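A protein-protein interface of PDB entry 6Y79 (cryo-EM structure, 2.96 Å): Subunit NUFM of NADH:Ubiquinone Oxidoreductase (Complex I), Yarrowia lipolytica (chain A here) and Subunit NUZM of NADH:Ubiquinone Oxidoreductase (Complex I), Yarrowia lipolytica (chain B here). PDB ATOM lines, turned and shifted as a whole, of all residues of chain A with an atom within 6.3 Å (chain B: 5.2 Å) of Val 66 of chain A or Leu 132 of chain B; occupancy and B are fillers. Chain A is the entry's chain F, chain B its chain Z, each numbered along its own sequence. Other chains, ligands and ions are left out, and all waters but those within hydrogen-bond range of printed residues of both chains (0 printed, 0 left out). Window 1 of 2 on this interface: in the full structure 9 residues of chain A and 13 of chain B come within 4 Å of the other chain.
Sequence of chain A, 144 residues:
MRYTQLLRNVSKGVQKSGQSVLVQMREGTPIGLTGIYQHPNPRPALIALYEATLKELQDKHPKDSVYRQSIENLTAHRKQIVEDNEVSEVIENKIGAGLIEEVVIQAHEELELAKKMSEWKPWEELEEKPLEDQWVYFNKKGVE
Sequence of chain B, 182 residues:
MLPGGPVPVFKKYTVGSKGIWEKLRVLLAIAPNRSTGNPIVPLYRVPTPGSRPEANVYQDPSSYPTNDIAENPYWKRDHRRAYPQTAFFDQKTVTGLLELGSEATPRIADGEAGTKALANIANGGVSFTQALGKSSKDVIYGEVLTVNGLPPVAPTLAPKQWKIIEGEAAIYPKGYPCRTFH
O of Lys 63 of chain A lies within hydrogen-bond range of NE2 of Gln 69 of chain A, 3.3 Å away.
The backbone carbonyl oxygen (O) of Ile 140 of chain B sits at hydrogen-bond distance from the backbone NH (N) of Leu 145 of chain B (2.9 Å).
The backbone carbonyl oxygen (O) of Val 66 of chain A is in hydrogen-bond range of the side-chain hydroxyl (OG) of Ser 70 of chain A, 3.4 Å away.
O of Leu 132 of chain B is in hydrogen-bond range of OG of Ser 135 of chain B.
CD2 of Leu 132 of chain B touches CG2 of Val 66 of chain A (3.98 Å).
CG1 of Val 66 of chain A touches CG1 of Val 144 of chain B, at 3.7 Å.
Val 66 of chain A touches Leu 145 of chain B.
Gln 69 of chain A touches Ile 140 of chain B (OE1 to CG2, 3.4 Å).
Of the printed residues of chain B, Gln 69 of chain A touches Ile 140.
Of the printed residues of chain A, Leu 132 of chain B touches Val 66.
Of the printed residues of chain A, Ile 140 of chain B touches Gln 69 (3.4 Å).
Of the printed residues of chain A, Val 144 of chain B touches Val 66 (3.7 Å).
Printed residues of chain A within 4 Å of Leu 145 of chain B: Val 66.
The nearest printed residue of chain B that does not touch Val 66 of chain A is Ile 140 of chain B (4.8 Å).
The nearest printed residue of chain A that does not touch Leu 132 of chain B is Asp 64 of chain A (5.0 Å).
Of the 12 printed residues of chain B, 4 touch a printed residue of chain A.
Among the printed residues, 4 pairs touch across the chains.
Among the printed residues, no Asp or Glu carboxylate lies within 4 Å of a Lys or Arg side-chain nitrogen of the other chain.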
ATOM      1  N   PRO A  62       9.735  16.599  -5.570  1.00  0.00           N
ATOM      2  CA  PRO A  62       8.917  17.415  -4.661  1.00  0.00           C
ATOM      3  C   PRO A  62       8.444  16.600  -3.469  1.00  0.00           C
ATOM      4  O   PRO A  62       8.093  15.431  -3.601  1.00  0.00           O
ATOM      5  CB  PRO A  62       7.728  17.834  -5.531  1.00  0.00           C
ATOM      6  CG  PRO A  62       8.184  17.629  -6.912  1.00  0.00           C
ATOM      7  CD  PRO A  62       9.071  16.438  -6.867  1.00  0.00           C
ATOM      8  N   LYS A  63       8.401  17.229  -2.299  1.00  0.00           N
ATOM      9  CA  LYS A  63       8.147  16.464  -1.081  1.00  0.00           C
ATOM     10  C   LYS A  63       6.696  16.027  -0.918  1.00  0.00           C
ATOM     11  O   LYS A  63       6.413  15.253   0.003  1.00  0.00           O
ATOM     12  CB  LYS A  63       8.570  17.251   0.158  1.00  0.00           C
ATOM     13  CG  LYS A  63       8.093  18.671   0.214  1.00  0.00           C
ATOM     14  CD  LYS A  63       9.039  19.490   1.078  1.00  0.00           C
ATOM     15  CE  LYS A  63      10.495  19.286   0.663  1.00  0.00           C
ATOM     16  NZ  LYS A  63      11.425  20.191   1.369  1.00  0.00           N
ATOM     17  N   ASP A  64       5.764  16.493  -1.761  1.00  0.00           N
ATOM     18  CA  ASP A  64       4.407  15.949  -1.722  1.00  0.00           C
ATOM     19  C   ASP A  64       4.314  14.596  -2.409  1.00  0.00           C
ATOM     20  O   ASP A  64       3.282  13.922  -2.282  1.00  0.00           O
ATOM     21  CB  ASP A  64       3.396  16.925  -2.350  1.00  0.00           C
ATOM     22  CG  ASP A  64       3.754  17.365  -3.763  1.00  0.00           C
ATOM     23  OD1 ASP A  64       4.684  18.191  -3.920  1.00  0.00           O
ATOM     24  OD2 ASP A  64       3.086  16.932  -4.736  1.00  0.00           O
ATOM     25  N   SER A  65       5.368  14.197  -3.142  1.00  0.00           N
ATOM     26  CA  SER A  65       5.348  12.970  -3.934  1.00  0.00           C
ATOM     27  C   SER A  65       5.228  11.754  -3.040  1.00  0.00           C
ATOM     28  O   SER A  65       5.896  11.660  -2.011  1.00  0.00           O
ATOM     29  CB  SER A  65       6.605  12.805  -4.753  1.00  0.00           C
ATOM     30  OG  SER A  65       6.898  13.912  -5.587  1.00  0.00           O
ATOM     31  N   VAL A  66       4.364  10.825  -3.435  1.00  0.00           N
ATOM     32  CA  VAL A  66       4.275   9.553  -2.735  1.00  0.00           C
ATOM     33  C   VAL A  66       5.509   8.707  -3.025  1.00  0.00           C
ATOM     34  O   VAL A  66       6.026   7.998  -2.146  1.00  0.00           O
ATOM     35  CB  VAL A  66       2.968   8.862  -3.146  1.00  0.00           C
ATOM     36  CG1 VAL A  66       2.831   7.550  -2.466  1.00  0.00           C
ATOM     37  CG2 VAL A  66       1.786   9.750  -2.793  1.00  0.00           C
ATOM     38  N   TYR A  67       6.015   8.810  -4.257  1.00  0.00           N
ATOM     39  CA  TYR A  67       7.237   8.130  -4.682  1.00  0.00           C
ATOM     40  C   TYR A  67       8.434   8.527  -3.822  1.00  0.00           C
ATOM     41  O   TYR A  67       9.155   7.666  -3.291  1.00  0.00           O
ATOM     42  CB  TYR A  67       7.487   8.467  -6.155  1.00  0.00           C
ATOM     43  CG  TYR A  67       8.715   7.854  -6.757  1.00  0.00           C
ATOM     44  CD1 TYR A  67       8.694   6.560  -7.233  1.00  0.00           C
ATOM     45  CD2 TYR A  67       9.894   8.577  -6.862  1.00  0.00           C
ATOM     46  CE1 TYR A  67       9.814   5.997  -7.791  1.00  0.00           C
ATOM     47  CE2 TYR A  67      11.020   8.019  -7.410  1.00  0.00           C
ATOM     48  CZ  TYR A  67      10.972   6.730  -7.874  1.00  0.00           C
ATOM     49  OH  TYR A  67      12.096   6.166  -8.420  1.00  0.00           O
ATOM     50  N   ARG A  68       8.642   9.837  -3.664  1.00  0.00           N
ATOM     51  CA  ARG A  68       9.761  10.351  -2.883  1.00  0.00           C
ATOM     52  C   ARG A  68       9.644   9.966  -1.415  1.00  0.00           C
ATOM     53  O   ARG A  68      10.631   9.525  -0.818  1.00  0.00           O
ATOM     54  CB  ARG A  68       9.838  11.868  -3.036  1.00  0.00           C
ATOM     55  CG  ARG A  68      10.935  12.566  -2.237  1.00  0.00           C
ATOM     56  CD  ARG A  68      10.704  14.054  -2.297  1.00  0.00           C
ATOM     57  NE  ARG A  68      11.777  14.914  -1.805  1.00  0.00           N
ATOM     58  CZ  ARG A  68      11.879  15.337  -0.551  1.00  0.00           C
ATOM     59  NH1 ARG A  68      10.987  14.961   0.352  1.00  0.00           N
ATOM     60  NH2 ARG A  68      12.872  16.135  -0.192  1.00  0.00           N
ATOM     61  N   GLN A  69       8.443  10.100  -0.831  1.00  0.00           N
ATOM     62  CA  GLN A  69       8.220   9.755   0.576  1.00  0.00           C
ATOM     63  C   GLN A  69       8.535   8.291   0.846  1.00  0.00           C
ATOM     64  O   GLN A  69       9.231   7.957   1.818  1.00  0.00           O
ATOM     65  CB  GLN A  69       6.772  10.043   0.976  1.00  0.00           C
ATOM     66  CG  GLN A  69       6.424  11.487   1.231  1.00  0.00           C
ATOM     67  CD  GLN A  69       4.943  11.669   1.449  1.00  0.00           C
ATOM     68  OE1 GLN A  69       4.217  10.700   1.650  1.00  0.00           O
ATOM     69  NE2 GLN A  69       4.477  12.906   1.354  1.00  0.00           N
ATOM     70  N   SER A  70       8.083   7.409  -0.045  1.00  0.00           N
ATOM     71  CA  SER A  70       8.295   5.985   0.165  1.00  0.00           C
ATOM     72  C   SER A  70       9.741   5.558  -0.034  1.00  0.00           C
ATOM     73  O   SER A  70      10.238   4.750   0.754  1.00  0.00           O
ATOM     74  CB  SER A  70       7.407   5.185  -0.768  1.00  0.00           C
ATOM     75  OG  SER A  70       7.922   5.205  -2.088  1.00  0.00           O
ATOM     76  N   ILE A  71      10.435   6.062  -1.057  1.00  0.00           N
ATOM     77  CA  ILE A  71      11.820   5.617  -1.209  1.00  0.00           C
ATOM     78  C   ILE A  71      12.732   6.287  -0.173  1.00  0.00           C
ATOM     79  O   ILE A  71      13.739   5.691   0.238  1.00  0.00           O
ATOM     80  CB  ILE A  71      12.287   5.818  -2.663  1.00  0.00           C
ATOM     81  CG1 ILE A  71      11.254   5.188  -3.597  1.00  0.00           C
ATOM     82  CG2 ILE A  71      13.650   5.171  -2.909  1.00  0.00           C
ATOM     83  CD1 ILE A  71      11.729   4.887  -4.999  1.00  0.00           C
ATOM     84  N   LEU B  98      -9.749   8.592  -2.231  1.00  0.00           N
ATOM     85  CA  LEU B  98      -8.815   9.373  -1.425  1.00  0.00           C
ATOM     86  C   LEU B  98      -9.492  10.533  -0.714  1.00  0.00           C
ATOM     87  O   LEU B  98      -9.041  10.946   0.359  1.00  0.00           O
ATOM     88  CB  LEU B  98      -7.687   9.927  -2.294  1.00  0.00           C
ATOM     89  CG  LEU B  98      -6.588   8.963  -2.721  1.00  0.00           C
ATOM     90  CD1 LEU B  98      -5.630   9.649  -3.673  1.00  0.00           C
ATOM     91  CD2 LEU B  98      -5.864   8.422  -1.510  1.00  0.00           C
ATOM     92  N   PHE B 128      -6.158  14.200  -9.586  1.00  0.00           N
ATOM     93  CA  PHE B 128      -5.617  13.151  -8.725  1.00  0.00           C
ATOM     94  C   PHE B 128      -4.398  13.620  -7.933  1.00  0.00           C
ATOM     95  O   PHE B 128      -4.255  13.278  -6.753  1.00  0.00           O
ATOM     96  CB  PHE B 128      -5.293  11.929  -9.590  1.00  0.00           C
ATOM     97  CG  PHE B 128      -4.708  10.767  -8.842  1.00  0.00           C
ATOM     98  CD1 PHE B 128      -5.473  10.021  -7.968  1.00  0.00           C
ATOM     99  CD2 PHE B 128      -3.401  10.392  -9.059  1.00  0.00           C
ATOM    100  CE1 PHE B 128      -4.923   8.943  -7.303  1.00  0.00           C
ATOM    101  CE2 PHE B 128      -2.852   9.322  -8.401  1.00  0.00           C
ATOM    102  CZ  PHE B 128      -3.614   8.595  -7.525  1.00  0.00           C
ATOM    103  N   THR B 129      -3.514  14.404  -8.550  1.00  0.00           N
ATOM    104  CA  THR B 129      -2.379  14.933  -7.802  1.00  0.00           C
ATOM    105  C   THR B 129      -2.817  16.056  -6.879  1.00  0.00           C
ATOM    106  O   THR B 129      -2.221  16.263  -5.813  1.00  0.00           O
ATOM    107  CB  THR B 129      -1.291  15.407  -8.755  1.00  0.00           C
ATOM    108  OG1 THR B 129      -1.826  16.399  -9.641  1.00  0.00           O
ATOM    109  CG2 THR B 129      -0.801  14.238  -9.563  1.00  0.00           C
ATOM    110  N   GLN B 130      -3.875  16.773  -7.262  1.00  0.00           N
ATOM    111  CA  GLN B 130      -4.531  17.667  -6.321  1.00  0.00           C
ATOM    112  C   GLN B 130      -5.091  16.902  -5.127  1.00  0.00           C
ATOM    113  O   GLN B 130      -4.994  17.383  -4.000  1.00  0.00           O
ATOM    114  CB  GLN B 130      -5.631  18.465  -7.024  1.00  0.00           C
ATOM    115  CG  GLN B 130      -5.087  19.496  -7.993  1.00  0.00           C
ATOM    116  CD  GLN B 130      -6.169  20.348  -8.624  1.00  0.00           C
ATOM    117  OE1 GLN B 130      -7.356  20.148  -8.375  1.00  0.00           O
ATOM    118  NE2 GLN B 130      -5.762  21.305  -9.452  1.00  0.00           N
ATOM    119  N   ALA B 131      -5.619  15.693  -5.343  1.00  0.00           N
ATOM    120  CA  ALA B 131      -6.096  14.873  -4.234  1.00  0.00           C
ATOM    121  C   ALA B 131      -4.946  14.384  -3.364  1.00  0.00           C
ATOM    122  O   ALA B 131      -5.098  14.259  -2.147  1.00  0.00           O
ATOM    123  CB  ALA B 131      -6.901  13.682  -4.759  1.00  0.00           C
ATOM    124  N   LEU B 132      -3.799  14.082  -3.973  1.00  0.00           N
ATOM    125  CA  LEU B 132      -2.647  13.646  -3.195  1.00  0.00           C
ATOM    126  C   LEU B 132      -2.070  14.786  -2.364  1.00  0.00           C
ATOM    127  O   LEU B 132      -1.558  14.551  -1.264  1.00  0.00           O
ATOM    128  CB  LEU B 132      -1.581  13.063  -4.121  1.00  0.00           C
ATOM    129  CG  LEU B 132      -1.914  11.742  -4.822  1.00  0.00           C
ATOM    130  CD1 LEU B 132      -0.905  11.438  -5.909  1.00  0.00           C
ATOM    131  CD2 LEU B 132      -1.966  10.609  -3.822  1.00  0.00           C
ATOM    132  N   GLY B 133      -2.147  16.017  -2.867  1.00  0.00           N
ATOM    133  CA  GLY B 133      -1.734  17.174  -2.093  1.00  0.00           C
ATOM    134  C   GLY B 133      -2.728  17.587  -1.022  1.00  0.00           C
ATOM    135  O   GLY B 133      -2.326  18.026   0.058  1.00  0.00           O
ATOM    136  N   LYS B 134      -4.028  17.468  -1.313  1.00  0.00           N
ATOM    137  CA  LYS B 134      -5.063  17.827  -0.345  1.00  0.00           C
ATOM    138  C   LYS B 134      -5.099  16.868   0.832  1.00  0.00           C
ATOM    139  O   LYS B 134      -5.444  17.271   1.946  1.00  0.00           O
ATOM    140  CB  LYS B 134      -6.446  17.841  -1.002  1.00  0.00           C
ATOM    141  CG  LYS B 134      -6.768  19.014  -1.909  1.00  0.00           C
ATOM    142  CD  LYS B 134      -8.124  18.801  -2.567  1.00  0.00           C
ATOM    143  CE  LYS B 134      -8.330  19.794  -3.690  1.00  0.00           C
ATOM    144  NZ  LYS B 134      -8.398  21.181  -3.175  1.00  0.00           N
ATOM    145  N   SER B 135      -4.761  15.604   0.608  1.00  0.00           N
ATOM    146  CA  SER B 135      -5.023  14.570   1.599  1.00  0.00           C
ATOM    147  C   SER B 135      -3.987  14.606   2.720  1.00  0.00           C
ATOM    148  O   SER B 135      -2.824  14.949   2.500  1.00  0.00           O
ATOM    149  CB  SER B 135      -5.044  13.199   0.916  1.00  0.00           C
ATOM    150  OG  SER B 135      -3.775  12.851   0.393  1.00  0.00           O
ATOM    151  N   ILE B 140      -2.232   9.363   3.946  1.00  0.00           N
ATOM    152  CA  ILE B 140      -1.208   8.908   3.010  1.00  0.00           C
ATOM    153  C   ILE B 140      -0.456   7.724   3.602  1.00  0.00           C
ATOM    154  O   ILE B 140      -0.159   6.746   2.908  1.00  0.00           O
ATOM    155  CB  ILE B 140      -0.270  10.069   2.617  1.00  0.00           C
ATOM    156  CG1 ILE B 140      -0.965  11.018   1.644  1.00  0.00           C
ATOM    157  CG2 ILE B 140       0.986   9.584   1.931  1.00  0.00           C
ATOM    158  CD1 ILE B 140      -0.232  12.334   1.453  1.00  0.00           C
ATOM    159  N   VAL B 144      -2.512   4.715   1.425  1.00  0.00           N
ATOM    160  CA  VAL B 144      -1.619   4.612   0.281  1.00  0.00           C
ATOM    161  C   VAL B 144      -0.380   3.806   0.638  1.00  0.00           C
ATOM    162  O   VAL B 144       0.019   2.894  -0.093  1.00  0.00           O
ATOM    163  CB  VAL B 144      -1.251   6.012  -0.227  1.00  0.00           C
ATOM    164  CG1 VAL B 144      -0.270   5.902  -1.357  1.00  0.00           C
ATOM    165  CG2 VAL B 144      -2.485   6.763  -0.684  1.00  0.00           C
ATOM    166  N   LEU B 145       0.229   4.108   1.775  1.00  0.00           N
ATOM    167  CA  LEU B 145       1.447   3.451   2.214  1.00  0.00           C
ATOM    168  C   LEU B 145       1.148   2.479   3.348  1.00  0.00           C
ATOM    169  O   LEU B 145       0.010   2.323   3.792  1.00  0.00           O
ATOM    170  CB  LEU B 145       2.486   4.476   2.676  1.00  0.00           C
ATOM    171  CG  LEU B 145       3.385   5.252   1.714  1.00  0.00           C
ATOM    172  CD1 LEU B 145       2.610   6.268   0.965  1.00  0.00           C
ATOM    173  CD2 LEU B 145       4.422   5.974   2.503  1.00  0.00           C
